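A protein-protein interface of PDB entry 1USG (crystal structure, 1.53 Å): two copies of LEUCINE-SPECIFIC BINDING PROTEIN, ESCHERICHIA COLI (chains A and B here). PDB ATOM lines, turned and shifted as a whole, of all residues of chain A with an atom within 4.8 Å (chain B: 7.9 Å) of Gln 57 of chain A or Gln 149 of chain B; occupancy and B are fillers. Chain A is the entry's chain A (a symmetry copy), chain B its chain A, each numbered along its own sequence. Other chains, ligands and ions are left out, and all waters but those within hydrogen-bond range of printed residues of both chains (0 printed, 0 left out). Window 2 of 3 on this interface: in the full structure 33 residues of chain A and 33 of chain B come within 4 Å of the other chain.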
ATOM      1  N   ASP A  50     -15.060  27.506  24.148  1.00  0.00           N
ATOM      2  CA  ASP A  50     -14.030  28.408  23.670  1.00  0.00           C
ATOM      3  C   ASP A  50     -13.539  27.956  22.302  1.00  0.00           C
ATOM      4  O   ASP A  50     -12.969  26.882  22.242  1.00  0.00           O
ATOM      5  CB  ASP A  50     -12.872  28.423  24.668  1.00  0.00           C
ATOM      6  CG  ASP A  50     -11.719  29.291  24.225  1.00  0.00           C
ATOM      7  OD1 ASP A  50     -10.558  29.027  24.692  1.00  0.00           O
ATOM      8  OD2 ASP A  50     -11.907  30.265  23.464  1.00  0.00           O
ATOM      9  N   ASP A  51     -13.735  28.759  21.246  1.00  0.00           N
ATOM     10  CA  ASP A  51     -13.093  28.439  19.966  1.00  0.00           C
ATOM     11  C   ASP A  51     -11.856  29.279  19.676  1.00  0.00           C
ATOM     12  O   ASP A  51     -11.231  29.146  18.610  1.00  0.00           O
ATOM     13  CB  ASP A  51     -14.078  28.519  18.812  1.00  0.00           C
ATOM     14  CG  ASP A  51     -14.510  29.930  18.480  1.00  0.00           C
ATOM     15  OD1 ASP A  51     -14.092  30.916  19.144  1.00  0.00           O
ATOM     16  OD2 ASP A  51     -15.283  30.154  17.514  1.00  0.00           O
ATOM     17  N   ALA A  52     -11.477  30.123  20.617  1.00  0.00           N
ATOM     18  CA  ALA A  52     -10.331  31.013  20.484  1.00  0.00           C
ATOM     19  C   ALA A  52     -10.353  31.857  19.214  1.00  0.00           C
ATOM     20  O   ALA A  52      -9.310  32.363  18.795  1.00  0.00           O
ATOM     21  CB  ALA A  52      -8.998  30.195  20.578  1.00  0.00           C
ATOM     22  N   ASP A  54     -10.471  30.720  16.329  1.00  0.00           N
ATOM     23  CA  ASP A  54      -9.485  29.996  15.524  1.00  0.00           C
ATOM     24  C   ASP A  54     -10.276  29.025  14.681  1.00  0.00           C
ATOM     25  O   ASP A  54     -11.038  28.218  15.200  1.00  0.00           O
ATOM     26  CB  ASP A  54      -8.560  29.224  16.451  1.00  0.00           C
ATOM     27  CG  ASP A  54      -7.445  28.454  15.721  1.00  0.00           C
ATOM     28  OD1 ASP A  54      -6.817  27.578  16.362  1.00  0.00           O
ATOM     29  OD2 ASP A  54      -7.102  28.663  14.552  1.00  0.00           O
ATOM     30  N   PRO A  55     -10.153  29.093  13.367  1.00  0.00           N
ATOM     31  CA  PRO A  55     -10.945  28.214  12.504  1.00  0.00           C
ATOM     32  C   PRO A  55     -10.940  26.711  12.848  1.00  0.00           C
ATOM     33  O   PRO A  55     -11.979  26.053  12.854  1.00  0.00           O
ATOM     34  CB  PRO A  55     -10.324  28.468  11.116  1.00  0.00           C
ATOM     35  CG  PRO A  55      -9.826  29.868  11.168  1.00  0.00           C
ATOM     36  CD  PRO A  55      -9.328  30.050  12.596  1.00  0.00           C
ATOM     37  N   LYS A  56      -9.765  26.156  13.114  1.00  0.00           N
ATOM     38  CA  LYS A  56      -9.649  24.748  13.379  1.00  0.00           C
ATOM     39  C   LYS A  56     -10.389  24.398  14.674  1.00  0.00           C
ATOM     40  O   LYS A  56     -11.074  23.381  14.764  1.00  0.00           O
ATOM     41  CB  LYS A  56      -8.165  24.402  13.515  1.00  0.00           C
ATOM     42  CG  LYS A  56      -7.851  23.022  13.995  1.00  0.00           C
ATOM     43  CD  LYS A  56      -6.325  22.804  13.889  1.00  0.00           C
ATOM     44  CE  LYS A  56      -5.963  21.356  13.605  1.00  0.00           C
ATOM     45  NZ  LYS A  56      -4.635  20.991  14.193  1.00  0.00           N
ATOM     46  N   GLN A  57     -10.233  25.248  15.682  1.00  0.00           N
ATOM     47  CA  GLN A  57     -10.958  25.009  16.920  1.00  0.00           C
ATOM     48  C   GLN A  57     -12.464  25.214  16.803  1.00  0.00           C
ATOM     49  O   GLN A  57     -13.238  24.554  17.465  1.00  0.00           O
ATOM     50  CB  GLN A  57     -10.432  25.909  18.016  1.00  0.00           C
ATOM     51  CG  GLN A  57      -9.006  25.600  18.360  1.00  0.00           C
ATOM     52  CD  GLN A  57      -8.500  26.414  19.533  1.00  0.00           C
ATOM     53  OE1 GLN A  57      -9.091  26.400  20.606  1.00  0.00           O
ATOM     54  NE2 GLN A  57      -7.395  27.101  19.333  1.00  0.00           N
ATOM     55  N   ALA A  58     -12.876  26.125  15.942  1.00  0.00           N
ATOM     56  CA  ALA A  58     -14.297  26.344  15.684  1.00  0.00           C
ATOM     57  C   ALA A  58     -14.961  25.102  15.109  1.00  0.00           C
ATOM     58  O   ALA A  58     -16.101  24.760  15.417  1.00  0.00           O
ATOM     59  CB  ALA A  58     -14.479  27.501  14.722  1.00  0.00           C
ATOM     60  N   VAL A  59     -14.251  24.440  14.207  1.00  0.00           N
ATOM     61  CA  VAL A  59     -14.734  23.231  13.627  1.00  0.00           C
ATOM     62  C   VAL A  59     -14.788  22.109  14.659  1.00  0.00           C
ATOM     63  O   VAL A  59     -15.763  21.375  14.729  1.00  0.00           O
ATOM     64  CB  VAL A  59     -13.836  22.817  12.437  1.00  0.00           C
ATOM     65  CG1 VAL A  59     -14.185  21.462  11.948  1.00  0.00           C
ATOM     66  CG2 VAL A  59     -13.987  23.850  11.350  1.00  0.00           C
ATOM     67  N   ALA A  60     -13.757  22.016  15.503  1.00  0.00           N
ATOM     68  CA  ALA A  60     -13.804  21.045  16.597  1.00  0.00           C
ATOM     69  C   ALA A  60     -15.015  21.268  17.521  1.00  0.00           C
ATOM     70  O   ALA A  60     -15.717  20.341  17.903  1.00  0.00           O
ATOM     71  CB  ALA A  60     -12.533  21.079  17.393  1.00  0.00           C
ATOM     72  N   VAL A  61     -15.246  22.530  17.872  1.00  0.00           N
ATOM     73  CA  VAL A  61     -16.375  22.888  18.742  1.00  0.00           C
ATOM     74  C   VAL A  61     -17.707  22.542  18.065  1.00  0.00           C
ATOM     75  O   VAL A  61     -18.591  21.988  18.683  1.00  0.00           O
ATOM     76  CB  VAL A  61     -16.307  24.382  19.133  1.00  0.00           C
ATOM     77  CG1 VAL A  61     -17.654  24.893  19.618  1.00  0.00           C
ATOM     78  CG2 VAL A  61     -15.225  24.573  20.220  1.00  0.00           C
ATOM     79  N   PRO B 104      -3.304  30.657  13.784  1.00  0.00           N
ATOM     80  CA  PRO B 104      -2.041  29.945  13.505  1.00  0.00           C
ATOM     81  C   PRO B 104      -1.812  29.394  12.081  1.00  0.00           C
ATOM     82  O   PRO B 104      -0.670  29.369  11.639  1.00  0.00           O
ATOM     83  CB  PRO B 104      -2.062  28.780  14.508  1.00  0.00           C
ATOM     84  CG  PRO B 104      -2.865  29.315  15.661  1.00  0.00           C
ATOM     85  CD  PRO B 104      -3.910  30.230  15.061  1.00  0.00           C
ATOM     86  N   GLU B 105      -2.840  28.938  11.372  1.00  0.00           N
ATOM     87  CA  GLU B 105      -2.649  28.340  10.047  1.00  0.00           C
ATOM     88  C   GLU B 105      -2.114  29.312   9.003  1.00  0.00           C
ATOM     89  O   GLU B 105      -1.623  28.923   7.937  1.00  0.00           O
ATOM     90  CB  GLU B 105      -3.960  27.747   9.499  1.00  0.00           C
ATOM     91  CG  GLU B 105      -4.843  26.917  10.440  1.00  0.00           C
ATOM     92  CD  GLU B 105      -6.240  26.622   9.832  1.00  0.00           C
ATOM     93  OE1 GLU B 105      -6.578  27.206   8.760  1.00  0.00           O
ATOM     94  OE2 GLU B 105      -7.028  25.803  10.400  1.00  0.00           O
ATOM     95  N   ASP B 121      -0.749  32.975  20.776  1.00  0.00           N
ATOM     96  CA  ASP B 121      -1.270  32.703  22.121  1.00  0.00           C
ATOM     97  C   ASP B 121      -0.412  31.623  22.810  1.00  0.00           C
ATOM     98  O   ASP B 121      -0.189  31.676  23.991  1.00  0.00           O
ATOM     99  CB  ASP B 121      -2.716  32.220  21.962  1.00  0.00           C
ATOM    100  CG  ASP B 121      -3.470  32.177  23.250  1.00  0.00           C
ATOM    101  OD1 ASP B 121      -3.575  33.257  23.884  1.00  0.00           O
ATOM    102  OD2 ASP B 121      -3.986  31.097  23.644  1.00  0.00           O
ATOM    103  N   HIS B 145      -4.170  21.043  34.627  1.00  0.00           N
ATOM    104  CA  HIS B 145      -4.888  21.578  33.450  1.00  0.00           C
ATOM    105  C   HIS B 145      -6.297  20.965  33.463  1.00  0.00           C
ATOM    106  O   HIS B 145      -6.550  20.061  34.249  1.00  0.00           O
ATOM    107  CB  HIS B 145      -4.160  21.235  32.148  1.00  0.00           C
ATOM    108  CG  HIS B 145      -4.059  19.773  31.924  1.00  0.00           C
ATOM    109  ND1 HIS B 145      -5.115  19.017  31.453  1.00  0.00           N
ATOM    110  CD2 HIS B 145      -3.066  18.901  32.215  1.00  0.00           C
ATOM    111  CE1 HIS B 145      -4.771  17.744  31.466  1.00  0.00           C
ATOM    112  NE2 HIS B 145      -3.531  17.643  31.918  1.00  0.00           N
ATOM    113  N   ASP B 146      -7.175  21.468  32.612  1.00  0.00           N
ATOM    114  CA  ASP B 146      -8.588  21.026  32.553  1.00  0.00           C
ATOM    115  C   ASP B 146      -8.928  20.160  31.377  1.00  0.00           C
ATOM    116  O   ASP B 146     -10.101  19.944  31.108  1.00  0.00           O
ATOM    117  CB  ASP B 146      -9.512  22.238  32.580  1.00  0.00           C
ATOM    118  CG  ASP B 146      -9.445  23.068  31.324  1.00  0.00           C
ATOM    119  OD1 ASP B 146     -10.235  24.044  31.180  1.00  0.00           O
ATOM    120  OD2 ASP B 146      -8.628  22.801  30.414  1.00  0.00           O
ATOM    121  N   LYS B 147      -7.905  19.575  30.779  1.00  0.00           N
ATOM    122  CA  LYS B 147      -8.071  18.581  29.669  1.00  0.00           C
ATOM    123  C   LYS B 147      -8.593  19.157  28.343  1.00  0.00           C
ATOM    124  O   LYS B 147      -8.809  18.435  27.359  1.00  0.00           O
ATOM    125  CB  LYS B 147      -8.916  17.383  30.091  1.00  0.00           C
ATOM    126  CG  LYS B 147      -8.609  16.852  31.465  1.00  0.00           C
ATOM    127  CD  LYS B 147      -9.346  15.535  31.700  1.00  0.00           C
ATOM    128  CE  LYS B 147      -9.296  15.188  33.153  1.00  0.00           C
ATOM    129  NZ  LYS B 147     -10.180  14.049  33.535  1.00  0.00           N
ATOM    130  N   GLN B 148      -8.717  20.465  28.271  1.00  0.00           N
ATOM    131  CA  GLN B 148      -9.165  21.118  27.049  1.00  0.00           C
ATOM    132  C   GLN B 148      -7.934  21.614  26.281  1.00  0.00           C
ATOM    133  O   GLN B 148      -6.835  21.827  26.851  1.00  0.00           O
ATOM    134  CB  GLN B 148     -10.114  22.282  27.355  1.00  0.00           C
ATOM    135  CG  GLN B 148     -11.235  21.916  28.262  1.00  0.00           C
ATOM    136  CD  GLN B 148     -11.993  20.752  27.755  1.00  0.00           C
ATOM    137  OE1 GLN B 148     -12.610  20.823  26.688  1.00  0.00           O
ATOM    138  NE2 GLN B 148     -11.930  19.648  28.490  1.00  0.00           N
ATOM    139  N   GLN B 149      -8.078  21.851  24.984  1.00  0.00           N
ATOM    140  CA  GLN B 149      -6.927  22.152  24.131  1.00  0.00           C
ATOM    141  C   GLN B 149      -6.072  23.322  24.635  1.00  0.00           C
ATOM    142  O   GLN B 149      -4.841  23.243  24.645  1.00  0.00           O
ATOM    143  CB  GLN B 149      -7.359  22.464  22.684  1.00  0.00           C
ATOM    144  CG  GLN B 149      -7.755  21.268  21.851  1.00  0.00           C
ATOM    145  CD  GLN B 149      -8.780  21.643  20.782  1.00  0.00           C
ATOM    146  OE1 GLN B 149      -8.530  22.543  19.969  1.00  0.00           O
ATOM    147  NE2 GLN B 149      -9.939  20.961  20.786  1.00  0.00           N
ATOM    148  N   TYR B 150      -6.727  24.404  25.016  1.00  0.00           N
ATOM    149  CA  TYR B 150      -6.032  25.593  25.488  1.00  0.00           C
ATOM    150  C   TYR B 150      -5.137  25.326  26.686  1.00  0.00           C
ATOM    151  O   TYR B 150      -3.912  25.464  26.631  1.00  0.00           O
ATOM    152  CB  TYR B 150      -7.039  26.671  25.851  1.00  0.00           C
ATOM    153  CG  TYR B 150      -6.469  27.935  26.484  1.00  0.00           C
ATOM    154  CD1 TYR B 150      -5.696  28.828  25.739  1.00  0.00           C
ATOM    155  CD2 TYR B 150      -6.725  28.249  27.805  1.00  0.00           C
ATOM    156  CE1 TYR B 150      -5.213  29.991  26.304  1.00  0.00           C
ATOM    157  CE2 TYR B 150      -6.250  29.455  28.387  1.00  0.00           C
ATOM    158  CZ  TYR B 150      -5.502  30.309  27.605  1.00  0.00           C
ATOM    159  OH  TYR B 150      -5.034  31.503  28.110  1.00  0.00           O
ATOM    160  N   GLY B 151      -5.768  24.926  27.772  1.00  0.00           N
ATOM    161  CA  GLY B 151      -5.061  24.691  29.019  1.00  0.00           C
ATOM    162  C   GLY B 151      -4.083  23.532  28.973  1.00  0.00           C
ATOM    163  O   GLY B 151      -2.975  23.622  29.498  1.00  0.00           O
ATOM    164  N   GLU B 152      -4.463  22.405  28.390  1.00  0.00           N
ATOM    165  CA  GLU B 152      -3.567  21.287  28.374  1.00  0.00           C
ATOM    166  C   GLU B 152      -2.359  21.616  27.487  1.00  0.00           C
ATOM    167  O   GLU B 152      -1.235  21.215  27.791  1.00  0.00           O
ATOM    168  CB  GLU B 152      -4.272  20.006  27.923  1.00  0.00           C
ATOM    169  CG  GLU B 152      -3.407  18.773  28.059  1.00  0.00           C
ATOM    170  CD  GLU B 152      -4.145  17.471  27.845  1.00  0.00           C
ATOM    171  OE1 GLU B 152      -5.390  17.485  27.664  1.00  0.00           O
ATOM    172  OE2 GLU B 152      -3.451  16.429  27.862  1.00  0.00           O
ATOM    173  N   GLY B 153      -2.553  22.336  26.394  1.00  0.00           N
ATOM    174  CA  GLY B 153      -1.450  22.701  25.537  1.00  0.00           C
ATOM    175  C   GLY B 153      -0.443  23.513  26.305  1.00  0.00           C
ATOM    176  O   GLY B 153       0.760  23.298  26.237  1.00  0.00           O
ATOM    177  N   LEU B 154      -0.938  24.518  26.996  1.00  0.00           N
ATOM    178  CA  LEU B 154      -0.064  25.394  27.741  1.00  0.00           C
ATOM    179  C   LEU B 154       0.605  24.688  28.896  1.00  0.00           C
ATOM    180  O   LEU B 154       1.787  24.881  29.115  1.00  0.00           O
ATOM    181  CB  LEU B 154      -0.837  26.623  28.192  1.00  0.00           C
ATOM    182  CG  LEU B 154      -1.109  27.663  27.086  1.00  0.00           C
ATOM    183  CD1 LEU B 154      -2.188  28.635  27.476  1.00  0.00           C
ATOM    184  CD2 LEU B 154       0.124  28.426  26.718  1.00  0.00           C
ATOM    185  N   ALA B 155      -0.123  23.870  29.653  1.00  0.00           N
ATOM    186  CA  ALA B 155       0.475  23.103  30.740  1.00  0.00           C
ATOM    187  C   ALA B 155       1.541  22.170  30.238  1.00  0.00           C
ATOM    188  O   ALA B 155       2.569  22.032  30.877  1.00  0.00           O
ATOM    189  CB  ALA B 155      -0.579  22.360  31.452  1.00  0.00           C
ATOM    190  N   ARG B 156       1.337  21.562  29.078  1.00  0.00           N
ATOM    191  CA  ARG B 156       2.361  20.656  28.511  1.00  0.00           C
ATOM    192  C   ARG B 156       3.604  21.394  28.107  1.00  0.00           C
ATOM    193  O   ARG B 156       4.685  20.886  28.294  1.00  0.00           O
ATOM    194  CB  ARG B 156       1.804  19.837  27.356  1.00  0.00           C
ATOM    195  CG  ARG B 156       0.844  18.768  27.872  1.00  0.00           C
ATOM    196  CD  ARG B 156       0.239  17.784  26.871  1.00  0.00           C
ATOM    197  NE  ARG B 156      -0.434  16.677  27.582  1.00  0.00           N
ATOM    198  CZ  ARG B 156       0.204  15.693  28.242  1.00  0.00           C
ATOM    199  NH1 ARG B 156       1.523  15.631  28.253  1.00  0.00           N
ATOM    200  NH2 ARG B 156      -0.488  14.748  28.871  1.00  0.00           N
ATOM    201  N   GLY B 200      -3.107  25.425  33.612  1.00  0.00           N
ATOM    202  CA  GLY B 200      -3.542  25.719  32.240  1.00  0.00           C
ATOM    203  C   GLY B 200      -5.045  25.549  32.140  1.00  0.00           C
ATOM    204  O   GLY B 200      -5.560  24.431  32.218  1.00  0.00           O
ATOM    205  N   TYR B 202      -9.009  28.088  32.530  1.00  0.00           N
ATOM    206  CA  TYR B 202      -9.763  29.329  32.629  1.00  0.00           C
ATOM    207  C   TYR B 202     -10.090  29.750  34.027  1.00  0.00           C
ATOM    208  O   TYR B 202     -10.004  28.963  34.982  1.00  0.00           O
ATOM    209  CB  TYR B 202     -11.074  29.125  31.858  1.00  0.00           C
ATOM    210  CG  TYR B 202     -10.890  28.633  30.429  1.00  0.00           C
ATOM    211  CD1 TYR B 202     -10.402  29.463  29.473  1.00  0.00           C
ATOM    212  CD2 TYR B 202     -11.220  27.341  30.072  1.00  0.00           C
ATOM    213  CE1 TYR B 202     -10.224  29.010  28.137  1.00  0.00           C
ATOM    214  CE2 TYR B 202     -11.050  26.856  28.733  1.00  0.00           C
ATOM    215  CZ  TYR B 202     -10.553  27.718  27.794  1.00  0.00           C
ATOM    216  OH  TYR B 202     -10.377  27.217  26.516  1.00  0.00           O
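Gln 57 of chain A touches just one residue of chain B: Gln 149 (3.5 Å).
Gln 149 of chain B touches one residue of chain A.
No residue of chain B comes within 4 Å of Ala 58 of chain A.
Of the printed residues of chain A, Tyr 202 of chain B touches Asp 50.
Of the printed residues of chain A, Glu 105 of chain B touches Lys 56 (3.6 Å).
Of the printed residues of chain B, Asp 50 of chain A touches Tyr 202.
Gln 148 of chain B touches none of the printed residues of chain A.
Val 61 of chain A touches none of the printed residues of chain B.
The nearest residue of chain B that does not touch Gln 57 of chain A is Tyr 150 of chain B (5.4 Å).
OH of Tyr 202 of chain B is in hydrogen-bond range of OD1 of Asp 50 of chain A (2.6 Å).
No position is printed for both chains.
Asp 54 of chain A touches Pro 104 of chain B (OD2 to CD, 3.6 Å).
OE2 of Glu 105 of chain B touches CB of Lys 56 of chain A (3.6 Å).
Gln 57 of chain A touches Gln 149 of chain B.
The side-chain carboxylate of Asp 50 of chain A is in hydrogen-bond range of the backbone NH of Ala 52 of chain A, at 2.9 Å.
OD1 of Asp 54 of chain A lies within hydrogen-bond range of NE2 of Gln 57 of chain A (3.1 Å).
Hydrophobic or aromatic side chains of chain B within 4 Å of the printed part of chain A: Pro 104 and Tyr 202.
Along chain A the printed residues that touch a printed residue of chain B span positions 50 to 57.
Among the printed residues, 4 pairs touch across the chains.
Among the printed residues, no Asp or Glu carboxylate lies within 4 Å of a Lys or Arg side-chain nitrogen of the other chain.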
